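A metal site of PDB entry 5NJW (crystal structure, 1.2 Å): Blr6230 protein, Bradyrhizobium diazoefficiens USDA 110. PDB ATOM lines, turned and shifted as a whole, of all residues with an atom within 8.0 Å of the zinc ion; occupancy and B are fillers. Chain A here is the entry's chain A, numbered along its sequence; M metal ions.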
ATOM      1  N   LYS A 157      21.864   1.464  10.116  1.00  0.00           N
ATOM      2  CA  LYS A 157      21.264   1.912   8.877  1.00  0.00           C
ATOM      3  C   LYS A 157      22.387   2.423   7.966  1.00  0.00           C
ATOM      4  O   LYS A 157      23.533   2.578   8.406  1.00  0.00           O
ATOM      5  CB  LYS A 157      20.234   3.019   9.142  1.00  0.00           C
ATOM      6  CG  LYS A 157      18.911   2.517   9.715  1.00  0.00           C
ATOM      7  CD  LYS A 157      17.940   3.672   9.927  1.00  0.00           C
ATOM      8  CE  LYS A 157      18.489   4.638  10.952  1.00  0.00           C
ATOM      9  N   GLU A 158      22.031   2.729   6.729  1.00  0.00           N
ATOM     10  CA  GLU A 158      22.973   3.268   5.735  1.00  0.00           C
ATOM     11  C   GLU A 158      23.801   4.406   6.292  1.00  0.00           C
ATOM     12  O   GLU A 158      23.264   5.402   6.845  1.00  0.00           O
ATOM     13  CB  GLU A 158      22.207   3.783   4.518  1.00  0.00           C
ATOM     14  CG  GLU A 158      23.013   4.533   3.481  1.00  0.00           C
ATOM     15  CD  GLU A 158      24.003   3.694   2.729  1.00  0.00           C
ATOM     16  OE1 GLU A 158      23.838   2.453   2.593  1.00  0.00           O
ATOM     17  OE2 GLU A 158      24.908   4.310   2.167  1.00  0.00           O
ATOM     18  N   GLY A 159      25.120   4.277   6.142  1.00  0.00           N
ATOM     19  CA  GLY A 159      26.080   5.295   6.550  1.00  0.00           C
ATOM     20  C   GLY A 159      26.536   5.243   7.982  1.00  0.00           C
ATOM     21  O   GLY A 159      27.460   5.974   8.354  1.00  0.00           O
ATOM     22  N   THR A 170      31.980   1.125   7.846  1.00  0.00           N
ATOM     23  CA  THR A 170      30.770   1.853   7.495  1.00  0.00           C
ATOM     24  C   THR A 170      29.738   0.888   6.959  1.00  0.00           C
ATOM     25  O   THR A 170      30.009   0.087   6.049  1.00  0.00           O
ATOM     26  CB  THR A 170      31.061   2.925   6.434  1.00  0.00           C
ATOM     27  OG1 THR A 170      32.046   3.816   6.964  1.00  0.00           O
ATOM     28  CG2 THR A 170      29.800   3.718   6.081  1.00  0.00           C
ATOM     29  N   ALA A 171      28.525   0.988   7.509  1.00  0.00           N
ATOM     30  CA  ALA A 171      27.401   0.148   7.075  1.00  0.00           C
ATOM     31  C   ALA A 171      26.789   0.681   5.793  1.00  0.00           C
ATOM     32  O   ALA A 171      26.538   1.908   5.682  1.00  0.00           O
ATOM     33  CB  ALA A 171      26.315   0.126   8.132  1.00  0.00           C
ATOM     34  N   HIS A 172      26.501  -0.202   4.832  1.00  0.00           N
ATOM     35  CA  HIS A 172      25.732   0.129   3.657  1.00  0.00           C
ATOM     36  C   HIS A 172      24.515  -0.783   3.620  1.00  0.00           C
ATOM     37  O   HIS A 172      24.634  -2.013   3.708  1.00  0.00           O
ATOM     38  CB  HIS A 172      26.518  -0.052   2.387  1.00  0.00           C
ATOM     39  CG  HIS A 172      27.661   0.885   2.265  1.00  0.00           C
ATOM     40  ND1 HIS A 172      27.534   2.149   1.741  1.00  0.00           N
ATOM     41  CD2 HIS A 172      28.946   0.747   2.641  1.00  0.00           C
ATOM     42  CE1 HIS A 172      28.714   2.746   1.784  1.00  0.00           C
ATOM     43  NE2 HIS A 172      29.581   1.920   2.331  1.00  0.00           N
ATOM     44  N   ALA A 173      23.335  -0.199   3.447  1.00  0.00           N
ATOM     45  CA  ALA A 173      22.107  -0.986   3.358  1.00  0.00           C
ATOM     46  C   ALA A 173      21.997  -1.565   1.955  1.00  0.00           C
ATOM     47  O   ALA A 173      21.854  -0.832   0.982  1.00  0.00           O
ATOM     48  CB  ALA A 173      20.909  -0.113   3.676  1.00  0.00           C
ATOM     49  N   THR A 174      22.111  -2.890   1.851  1.00  0.00           N
ATOM     50  CA  THR A 174      22.060  -3.602   0.584  1.00  0.00           C
ATOM     51  C   THR A 174      21.032  -4.738   0.691  1.00  0.00           C
ATOM     52  O   THR A 174      21.390  -5.913   0.536  1.00  0.00           O
ATOM     53  CB  THR A 174      23.452  -4.123   0.205  1.00  0.00           C
ATOM     54  OG1 THR A 174      24.035  -4.787   1.328  1.00  0.00           O
ATOM     55  CG2 THR A 174      24.363  -2.974  -0.205  1.00  0.00           C
ATOM     56  N   SER A 183      26.143  -4.491   3.915  1.00  0.00           N
ATOM     57  CA  SER A 183      27.497  -4.598   3.377  1.00  0.00           C
ATOM     58  C   SER A 183      28.397  -3.629   4.124  1.00  0.00           C
ATOM     59  O   SER A 183      28.050  -2.475   4.307  1.00  0.00           O
ATOM     60  CB  SER A 183      27.523  -4.353   1.876  1.00  0.00           C
ATOM     61  OG  SER A 183      26.747  -5.300   1.182  1.00  0.00           O
ATOM     62  N   GLU A 185      31.983  -1.545   4.746  1.00  0.00           N
ATOM     63  CA  GLU A 185      33.148  -0.979   4.058  1.00  0.00           C
ATOM     64  C   GLU A 185      34.206  -0.571   5.064  1.00  0.00           C
ATOM     65  O   GLU A 185      33.911  -0.034   6.119  1.00  0.00           O
ATOM     66  CB  GLU A 185      32.727   0.234   3.265  1.00  0.00           C
ATOM     67  CG  GLU A 185      33.869   0.874   2.460  1.00  0.00           C
ATOM     68  CD  GLU A 185      33.399   1.988   1.563  1.00  0.00           C
ATOM     69  OE1 GLU A 185      32.186   2.233   1.433  1.00  0.00           O
ATOM     70  OE2 GLU A 185      34.275   2.666   0.974  1.00  0.00           O
ATOM     71  N   LEU A 198      35.028  -4.101   0.657  1.00  0.00           N
ATOM     72  CA  LEU A 198      33.590  -4.298   0.978  1.00  0.00           C
ATOM     73  C   LEU A 198      33.341  -5.755   1.355  1.00  0.00           C
ATOM     74  O   LEU A 198      33.577  -6.650   0.541  1.00  0.00           O
ATOM     75  CB  LEU A 198      32.681  -3.908  -0.185  1.00  0.00           C
ATOM     76  CG  LEU A 198      31.198  -3.864   0.206  1.00  0.00           C
ATOM     77  CD1 LEU A 198      30.919  -2.637   1.032  1.00  0.00           C
ATOM     78  CD2 LEU A 198      30.341  -3.838  -1.034  1.00  0.00           C
ATOM     79  N   LYS A 229      23.342  -0.219  -6.718  1.00  0.00           N
ATOM     80  CA  LYS A 229      24.214   0.381  -5.722  1.00  0.00           C
ATOM     81  C   LYS A 229      25.609  -0.259  -5.763  1.00  0.00           C
ATOM     82  O   LYS A 229      26.625   0.454  -5.761  1.00  0.00           O
ATOM     83  CB  LYS A 229      23.590   0.188  -4.345  1.00  0.00           C
ATOM     84  CG  LYS A 229      24.430   0.692  -3.193  1.00  0.00           C
ATOM     85  CD  LYS A 229      23.647   0.546  -1.900  1.00  0.00           C
ATOM     86  CE  LYS A 229      24.432   0.840  -0.651  1.00  0.00           C
ATOM     87  NZ  LYS A 229      24.773   2.264  -0.569  1.00  0.00           N
ATOM     88  N   MET A 233      29.647   1.536  -6.438  1.00  0.00           N
ATOM     89  CA  MET A 233      30.572   1.694  -5.324  1.00  0.00           C
ATOM     90  C   MET A 233      32.030   1.549  -5.769  1.00  0.00           C
ATOM     91  O   MET A 233      32.351   0.697  -6.570  1.00  0.00           O
ATOM     92  CB  MET A 233      30.282   0.684  -4.218  1.00  0.00           C
ATOM     93  CG  MET A 233      28.931   0.908  -3.566  1.00  0.00           C
ATOM     94  SD  MET A 233      28.497  -0.360  -2.381  1.00  0.00           S
ATOM     95  CE  MET A 233      29.663   0.177  -1.157  1.00  0.00           C
HETATM   96 ZN    ZN M   1      25.982   3.120   0.899  1.00  0.00          ZN
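A ring nitrogen (NE2) of His 172 is in hydrogen-bond range of the side-chain carboxylate of Glu 185 (2.8 Å). The side-chain carboxylate of Glu 158 lies within hydrogen-bond range of the backbone NH of Ala 173 (2.8 Å). The backbone NH of His 172 is in hydrogen-bond range of the backbone carbonyl oxygen of Ser 183, 2.8 Å away.
ND1 of His 172 binds the zinc ion, 2.0 Å away. The zinc ion is bound by the side-chain carboxylate (OE2) of Glu 158, at 2.0 Å. The side-chain amino group (NZ) of Lys 229 is bound to the zinc ion, at 2.1 Å. The zinc ion has three donor atoms within binding distance. Slightly farther from the zinc ion lies OE1 of Glu 158 (2.8 Å).
Within 4 Å of the zinc ion: Glu 158, His 172 and Lys 229.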
